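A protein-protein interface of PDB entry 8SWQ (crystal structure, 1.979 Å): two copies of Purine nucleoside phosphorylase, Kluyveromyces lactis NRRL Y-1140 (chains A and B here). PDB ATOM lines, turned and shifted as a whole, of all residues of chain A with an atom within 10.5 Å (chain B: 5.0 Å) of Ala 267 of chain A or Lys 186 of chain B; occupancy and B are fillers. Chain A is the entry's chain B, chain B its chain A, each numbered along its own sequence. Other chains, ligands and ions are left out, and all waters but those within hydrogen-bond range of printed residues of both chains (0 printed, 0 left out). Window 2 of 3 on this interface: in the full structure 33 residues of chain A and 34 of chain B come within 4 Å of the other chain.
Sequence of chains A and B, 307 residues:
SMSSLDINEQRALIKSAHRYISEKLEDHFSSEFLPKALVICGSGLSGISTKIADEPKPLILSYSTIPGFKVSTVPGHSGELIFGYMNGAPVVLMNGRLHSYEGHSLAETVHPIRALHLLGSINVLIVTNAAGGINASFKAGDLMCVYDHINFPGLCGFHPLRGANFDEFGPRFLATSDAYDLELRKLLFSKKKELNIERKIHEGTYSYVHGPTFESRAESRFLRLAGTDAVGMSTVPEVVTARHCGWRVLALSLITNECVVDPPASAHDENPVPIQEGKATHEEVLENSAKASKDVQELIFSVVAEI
Hydrophobic or aromatic side chains of chain A that line the printed part of chain B: Ala 267, His 268, Pro 272 and Ile 275. Printed residues of chain B that touch a printed residue of chain A: Leu 182, Arg 185, Lys 186, Phe 189 and Glu 203. Among the printed residues, no Asp or Glu carboxylate lies within 4 Å of a Lys or Arg side-chain nitrogen of the other chain.
The backbone NH (N) of His 268 of chain A is in hydrogen-bond range of the side-chain hydroxyl (OG) of Ser 266 of chain A, at 2.9 Å. NH2 of Arg 185 of chain B lies within salt-bridge range of OE2 of Glu 203 of chain B. The side-chain hydroxyl (OG) of Ser 190 of chain B is in hydrogen-bond range of the backbone carbonyl oxygen (O) of Lys 186 of chain B (3.2 Å). The backbone NH (N) of Ser 266 of chain A lies within hydrogen-bond range of the side-chain carboxylate (OD2) of Asp 269 of chain A (2.9 Å).
The side-chain carboxylate (OE2) of Glu 203 of chain B is in hydrogen-bond range of the backbone NH (N) of Ala 267 of chain A, at 2.9 Å. O of Ala 265 of chain A sits at hydrogen-bond distance from NH2 of Arg 185 of chain B (2.9 Å). The side-chain hydroxyl (OG) of Ser 266 of chain A is in hydrogen-bond range of the side-chain carboxylate (OE1) of Glu 203 of chain B (2.9 Å). The side-chain amino group (NZ) of Lys 186 of chain B sits at hydrogen-bond distance from the backbone carbonyl oxygen (O) of Ala 267 of chain A (3.3 Å).
No position is printed for both chains.
Among the printed residues, pairs that only touch across the chains: Ala 265 of chain A with Leu 182 of chain B (3.8 Å), Ser 266 of chain A with Leu 182 of chain B (3.7 Å), Ser 266 of chain A with Arg 185 of chain B (3.99 Å), Ala 267 of chain A with Arg 185 of chain B (3.6 Å), Ala 267 of chain A with Phe 189 of chain B (3.6 Å), His 268 of chain A with Phe 189 of chain B (3.7 Å), His 268 of chain A with Glu 203 of chain B (3.9 Å), Pro 272 of chain A with Leu 182 of chain B (3.7 Å) and Ile 275 of chain A with Leu 182 of chain B (3.99 Å).
Pro 264 of chain A touches none of the printed residues of chain B. Of the printed residues of chain B, Ala 265 of chain A touches Leu 182 (3.8 Å) and Arg 185 (2.9 Å). Printed residues of chain B within 4 Å of Ser 266 of chain A: Leu 182 (3.7 Å), Arg 185 (3.99 Å) and Glu 203 (2.9 Å). Of the printed residues of chain B, His 268 of chain A touches Phe 189 and Glu 203. Glu 270 of chain A touches none of the printed residues of chain B. Of the printed residues of chain B, Pro 272 of chain A touches Leu 182. No residue of chain A comes within 4 Å of Glu 183 of chain B. Of the printed residues of chain A, Lys 186 of chain B touches Ala 267 (3.3 Å). No residue of chain A comes within 4 Å of Leu 187 of chain B. Phe 189 of chain B touches two residues of chain A. No residue of chain A comes within 4 Å of Ser 190 of chain B. Of the printed residues of chain A, Glu 203 of chain B touches Ser 266 (2.9 Å), Ala 267 (2.9 Å) and His 268 (3.9 Å).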
ATOM      1  N   PRO A 263     -16.929  28.577  -8.123  1.00  0.00           N
ATOM      2  CA  PRO A 263     -15.918  29.453  -7.521  1.00  0.00           C
ATOM      3  C   PRO A 263     -14.871  28.600  -6.806  1.00  0.00           C
ATOM      4  O   PRO A 263     -15.212  27.542  -6.276  1.00  0.00           O
ATOM      5  CB  PRO A 263     -16.718  30.264  -6.482  1.00  0.00           C
ATOM      6  CG  PRO A 263     -18.162  30.156  -6.927  1.00  0.00           C
ATOM      7  CD  PRO A 263     -18.279  28.800  -7.565  1.00  0.00           C
ATOM      8  N   PRO A 264     -13.610  29.051  -6.786  1.00  0.00           N
ATOM      9  CA  PRO A 264     -12.570  28.234  -6.159  1.00  0.00           C
ATOM     10  C   PRO A 264     -12.747  28.220  -4.645  1.00  0.00           C
ATOM     11  O   PRO A 264     -13.493  29.047  -4.097  1.00  0.00           O
ATOM     12  CB  PRO A 264     -11.281  28.978  -6.517  1.00  0.00           C
ATOM     13  CG  PRO A 264     -11.718  30.435  -6.605  1.00  0.00           C
ATOM     14  CD  PRO A 264     -13.147  30.416  -7.104  1.00  0.00           C
ATOM     15  N   ALA A 265     -12.067  27.298  -3.974  1.00  0.00           N
ATOM     16  CA  ALA A 265     -12.140  27.213  -2.511  1.00  0.00           C
ATOM     17  C   ALA A 265     -11.794  28.552  -1.847  1.00  0.00           C
ATOM     18  O   ALA A 265     -10.834  29.218  -2.238  1.00  0.00           O
ATOM     19  CB  ALA A 265     -11.212  26.126  -2.004  1.00  0.00           C
ATOM     20  N   SER A 266     -12.575  28.945  -0.843  1.00  0.00           N
ATOM     21  CA  SER A 266     -12.280  30.154  -0.084  1.00  0.00           C
ATOM     22  C   SER A 266     -11.211  29.862   0.962  1.00  0.00           C
ATOM     23  O   SER A 266     -11.127  28.741   1.479  1.00  0.00           O
ATOM     24  CB  SER A 266     -13.539  30.647   0.633  1.00  0.00           C
ATOM     25  OG  SER A 266     -13.189  31.516   1.702  1.00  0.00           O
ATOM     26  N   ALA A 267     -10.423  30.874   1.312  1.00  0.00           N
ATOM     27  CA  ALA A 267      -9.442  30.716   2.379  1.00  0.00           C
ATOM     28  C   ALA A 267     -10.116  30.447   3.714  1.00  0.00           C
ATOM     29  O   ALA A 267      -9.469  30.000   4.671  1.00  0.00           O
ATOM     30  CB  ALA A 267      -8.554  31.947   2.479  1.00  0.00           C
ATOM     31  N   HIS A 268     -11.421  30.702   3.786  1.00  0.00           N
ATOM     32  CA  HIS A 268     -12.149  30.523   5.040  1.00  0.00           C
ATOM     33  C   HIS A 268     -12.842  29.161   5.125  1.00  0.00           C
ATOM     34  O   HIS A 268     -13.427  28.832   6.160  1.00  0.00           O
ATOM     35  CB  HIS A 268     -13.187  31.634   5.234  1.00  0.00           C
ATOM     36  CG  HIS A 268     -12.652  33.013   4.998  1.00  0.00           C
ATOM     37  ND1 HIS A 268     -11.810  33.645   5.885  1.00  0.00           N
ATOM     38  CD2 HIS A 268     -12.856  33.885   3.982  1.00  0.00           C
ATOM     39  CE1 HIS A 268     -11.508  34.846   5.422  1.00  0.00           C
ATOM     40  NE2 HIS A 268     -12.131  35.018   4.271  1.00  0.00           N
ATOM     41  N   ASP A 269     -12.787  28.385   4.047  1.00  0.00           N
ATOM     42  CA  ASP A 269     -13.438  27.068   4.003  1.00  0.00           C
ATOM     43  C   ASP A 269     -12.635  26.089   4.854  1.00  0.00           C
ATOM     44  O   ASP A 269     -11.439  25.946   4.650  1.00  0.00           O
ATOM     45  CB  ASP A 269     -13.493  26.528   2.558  1.00  0.00           C
ATOM     46  CG  ASP A 269     -14.490  27.277   1.669  1.00  0.00           C
ATOM     47  OD1 ASP A 269     -15.365  27.979   2.220  1.00  0.00           O
ATOM     48  OD2 ASP A 269     -14.402  27.152   0.412  1.00  0.00           O
ATOM     49  N   GLU A 270     -13.259  25.405   5.804  1.00  0.00           N
ATOM     50  CA  GLU A 270     -12.485  24.418   6.566  1.00  0.00           C
ATOM     51  C   GLU A 270     -12.503  23.051   5.892  1.00  0.00           C
ATOM     52  O   GLU A 270     -11.769  22.144   6.290  1.00  0.00           O
ATOM     53  CB  GLU A 270     -12.916  24.342   8.040  1.00  0.00           C
ATOM     54  CG  GLU A 270     -14.396  24.122   8.255  1.00  0.00           C
ATOM     55  CD  GLU A 270     -14.719  23.641   9.663  1.00  0.00           C
ATOM     56  OE1 GLU A 270     -15.325  22.546   9.775  1.00  0.00           O
ATOM     57  OE2 GLU A 270     -14.368  24.346  10.649  1.00  0.00           O
ATOM     58  N   ASN A 271     -13.347  22.906   4.873  1.00  0.00           N
ATOM     59  CA  ASN A 271     -13.382  21.689   4.075  1.00  0.00           C
ATOM     60  C   ASN A 271     -13.356  22.013   2.594  1.00  0.00           C
ATOM     61  O   ASN A 271     -14.335  21.764   1.897  1.00  0.00           O
ATOM     62  CB  ASN A 271     -14.643  20.878   4.385  1.00  0.00           C
ATOM     63  CG  ASN A 271     -14.686  20.423   5.811  1.00  0.00           C
ATOM     64  OD1 ASN A 271     -15.303  21.062   6.668  1.00  0.00           O
ATOM     65  ND2 ASN A 271     -13.991  19.332   6.093  1.00  0.00           N
ATOM     66  N   PRO A 272     -12.231  22.566   2.108  1.00  0.00           N
ATOM     67  CA  PRO A 272     -12.193  23.054   0.727  1.00  0.00           C
ATOM     68  C   PRO A 272     -12.077  21.950  -0.323  1.00  0.00           C
ATOM     69  O   PRO A 272     -11.420  20.925  -0.114  1.00  0.00           O
ATOM     70  CB  PRO A 272     -10.934  23.930   0.698  1.00  0.00           C
ATOM     71  CG  PRO A 272     -10.029  23.331   1.742  1.00  0.00           C
ATOM     72  CD  PRO A 272     -10.960  22.803   2.826  1.00  0.00           C
ATOM     73  N   VAL A 273     -12.743  22.170  -1.449  1.00  0.00           N
ATOM     74  CA  VAL A 273     -12.497  21.410  -2.663  1.00  0.00           C
ATOM     75  C   VAL A 273     -11.181  21.927  -3.248  1.00  0.00           C
ATOM     76  O   VAL A 273     -11.032  23.129  -3.452  1.00  0.00           O
ATOM     77  CB  VAL A 273     -13.618  21.656  -3.699  1.00  0.00           C
ATOM     78  CG1 VAL A 273     -13.343  20.878  -4.980  1.00  0.00           C
ATOM     79  CG2 VAL A 273     -14.985  21.280  -3.120  1.00  0.00           C
ATOM     80  N   ILE A 275      -8.321  23.273  -5.535  1.00  0.00           N
ATOM     81  CA  ILE A 275      -8.478  24.066  -6.756  1.00  0.00           C
ATOM     82  C   ILE A 275      -8.035  23.325  -8.007  1.00  0.00           C
ATOM     83  O   ILE A 275      -8.428  23.694  -9.125  1.00  0.00           O
ATOM     84  CB  ILE A 275      -7.772  25.456  -6.660  1.00  0.00           C
ATOM     85  CG1 ILE A 275      -6.254  25.308  -6.622  1.00  0.00           C
ATOM     86  CG2 ILE A 275      -8.256  26.221  -5.421  1.00  0.00           C
ATOM     87  CD1 ILE A 275      -5.519  26.661  -6.433  1.00  0.00           C
ATOM     88  N   LEU B 182      -4.368  27.972  -2.846  1.00  0.00           N
ATOM     89  CA  LEU B 182      -5.170  28.077  -1.629  1.00  0.00           C
ATOM     90  C   LEU B 182      -4.304  28.325  -0.393  1.00  0.00           C
ATOM     91  O   LEU B 182      -4.630  29.176   0.436  1.00  0.00           O
ATOM     92  CB  LEU B 182      -6.055  26.830  -1.449  1.00  0.00           C
ATOM     93  CG  LEU B 182      -6.873  26.796  -0.152  1.00  0.00           C
ATOM     94  CD1 LEU B 182      -7.880  27.947  -0.135  1.00  0.00           C
ATOM     95  CD2 LEU B 182      -7.573  25.455   0.001  1.00  0.00           C
ATOM     96  N   GLU B 183      -3.187  27.616  -0.267  1.00  0.00           N
ATOM     97  CA  GLU B 183      -2.402  27.729   0.967  1.00  0.00           C
ATOM     98  C   GLU B 183      -1.777  29.105   1.160  1.00  0.00           C
ATOM     99  O   GLU B 183      -1.634  29.577   2.290  1.00  0.00           O
ATOM    100  CB  GLU B 183      -1.358  26.605   1.085  1.00  0.00           C
ATOM    101  CG  GLU B 183      -1.956  25.249   1.480  1.00  0.00           C
ATOM    102  CD  GLU B 183      -3.004  25.344   2.599  1.00  0.00           C
ATOM    103  OE1 GLU B 183      -4.218  25.302   2.284  1.00  0.00           O
ATOM    104  OE2 GLU B 183      -2.622  25.453   3.793  1.00  0.00           O
ATOM    105  N   LEU B 184      -1.431  29.773   0.064  1.00  0.00           N
ATOM    106  CA  LEU B 184      -0.900  31.125   0.171  1.00  0.00           C
ATOM    107  C   LEU B 184      -1.981  32.119   0.591  1.00  0.00           C
ATOM    108  O   LEU B 184      -1.709  33.069   1.322  1.00  0.00           O
ATOM    109  CB  LEU B 184      -0.285  31.563  -1.167  1.00  0.00           C
ATOM    110  CG  LEU B 184       1.035  30.871  -1.520  1.00  0.00           C
ATOM    111  CD1 LEU B 184       1.496  31.302  -2.925  1.00  0.00           C
ATOM    112  CD2 LEU B 184       2.079  31.231  -0.492  1.00  0.00           C
ATOM    113  N   ARG B 185      -3.207  31.925   0.121  1.00  0.00           N
ATOM    114  CA  ARG B 185      -4.307  32.801   0.540  1.00  0.00           C
ATOM    115  C   ARG B 185      -4.622  32.589   2.017  1.00  0.00           C
ATOM    116  O   ARG B 185      -4.937  33.536   2.745  1.00  0.00           O
ATOM    117  CB  ARG B 185      -5.563  32.572  -0.320  1.00  0.00           C
ATOM    118  CG  ARG B 185      -5.373  33.031  -1.774  1.00  0.00           C
ATOM    119  CD  ARG B 185      -6.655  32.986  -2.598  1.00  0.00           C
ATOM    120  NE  ARG B 185      -6.916  31.668  -3.173  1.00  0.00           N
ATOM    121  CZ  ARG B 185      -7.923  30.871  -2.830  1.00  0.00           C
ATOM    122  NH1 ARG B 185      -8.067  29.700  -3.438  1.00  0.00           N
ATOM    123  NH2 ARG B 185      -8.797  31.243  -1.895  1.00  0.00           N
ATOM    124  N   LYS B 186      -4.518  31.350   2.471  1.00  0.00           N
ATOM    125  CA  LYS B 186      -4.731  31.073   3.892  1.00  0.00           C
ATOM    126  C   LYS B 186      -3.605  31.687   4.722  1.00  0.00           C
ATOM    127  O   LYS B 186      -3.831  32.209   5.827  1.00  0.00           O
ATOM    128  CB  LYS B 186      -4.817  29.564   4.132  1.00  0.00           C
ATOM    129  CG  LYS B 186      -6.158  28.936   3.723  1.00  0.00           C
ATOM    130  CD  LYS B 186      -6.279  27.485   4.198  1.00  0.00           C
ATOM    131  CE  LYS B 186      -6.235  27.385   5.724  1.00  0.00           C
ATOM    132  NZ  LYS B 186      -7.328  28.157   6.398  1.00  0.00           N
ATOM    133  N   LEU B 187      -2.392  31.641   4.178  1.00  0.00           N
ATOM    134  CA  LEU B 187      -1.238  32.269   4.826  1.00  0.00           C
ATOM    135  C   LEU B 187      -1.474  33.774   4.964  1.00  0.00           C
ATOM    136  O   LEU B 187      -1.284  34.350   6.034  1.00  0.00           O
ATOM    137  CB  LEU B 187       0.049  31.990   4.028  1.00  0.00           C
ATOM    138  CG  LEU B 187       1.279  32.739   4.561  1.00  0.00           C
ATOM    139  CD1 LEU B 187       1.576  32.294   6.010  1.00  0.00           C
ATOM    140  CD2 LEU B 187       2.486  32.494   3.667  1.00  0.00           C
ATOM    141  N   LEU B 188      -1.904  34.413   3.879  1.00  0.00           N
ATOM    142  CA  LEU B 188      -2.226  35.841   3.937  1.00  0.00           C
ATOM    143  C   LEU B 188      -3.209  36.166   5.059  1.00  0.00           C
ATOM    144  O   LEU B 188      -2.976  37.073   5.859  1.00  0.00           O
ATOM    145  CB  LEU B 188      -2.767  36.332   2.589  1.00  0.00           C
ATOM    146  CG  LEU B 188      -3.243  37.785   2.574  1.00  0.00           C
ATOM    147  CD1 LEU B 188      -2.045  38.754   2.705  1.00  0.00           C
ATOM    148  CD2 LEU B 188      -4.008  38.074   1.297  1.00  0.00           C
ATOM    149  N   PHE B 189      -4.312  35.425   5.137  1.00  0.00           N
ATOM    150  CA  PHE B 189      -5.287  35.693   6.186  1.00  0.00           C
ATOM    151  C   PHE B 189      -4.742  35.367   7.582  1.00  0.00           C
ATOM    152  O   PHE B 189      -5.098  36.032   8.545  1.00  0.00           O
ATOM    153  CB  PHE B 189      -6.625  34.975   5.915  1.00  0.00           C
ATOM    154  CG  PHE B 189      -7.456  35.624   4.826  1.00  0.00           C
ATOM    155  CD1 PHE B 189      -8.292  36.694   5.119  1.00  0.00           C
ATOM    156  CD2 PHE B 189      -7.397  35.162   3.509  1.00  0.00           C
ATOM    157  CE1 PHE B 189      -9.053  37.306   4.114  1.00  0.00           C
ATOM    158  CE2 PHE B 189      -8.159  35.762   2.497  1.00  0.00           C
ATOM    159  CZ  PHE B 189      -8.983  36.844   2.806  1.00  0.00           C
ATOM    160  N   SER B 190      -3.875  34.363   7.703  1.00  0.00           N
ATOM    161  CA  SER B 190      -3.255  34.083   9.007  1.00  0.00           C
ATOM    162  C   SER B 190      -2.397  35.252   9.480  1.00  0.00           C
ATOM    163  O   SER B 190      -2.334  35.561  10.683  1.00  0.00           O
ATOM    164  CB  SER B 190      -2.383  32.825   8.961  1.00  0.00           C
ATOM    165  OG  SER B 190      -3.178  31.665   8.878  1.00  0.00           O
ATOM    166  N   GLU B 203     -12.281  38.399  -0.651  1.00  0.00           N
ATOM    167  CA  GLU B 203     -11.740  37.440  -1.606  1.00  0.00           C
ATOM    168  C   GLU B 203     -12.616  37.574  -2.834  1.00  0.00           C
ATOM    169  O   GLU B 203     -13.839  37.634  -2.700  1.00  0.00           O
ATOM    170  CB  GLU B 203     -11.870  36.011  -1.062  1.00  0.00           C
ATOM    171  CG  GLU B 203     -10.565  35.381  -0.623  1.00  0.00           C
ATOM    172  CD  GLU B 203     -10.734  33.922  -0.223  1.00  0.00           C
ATOM    173  OE1 GLU B 203     -11.844  33.551   0.222  1.00  0.00           O
ATOM    174  OE2 GLU B 203      -9.762  33.147  -0.366  1.00  0.00           O
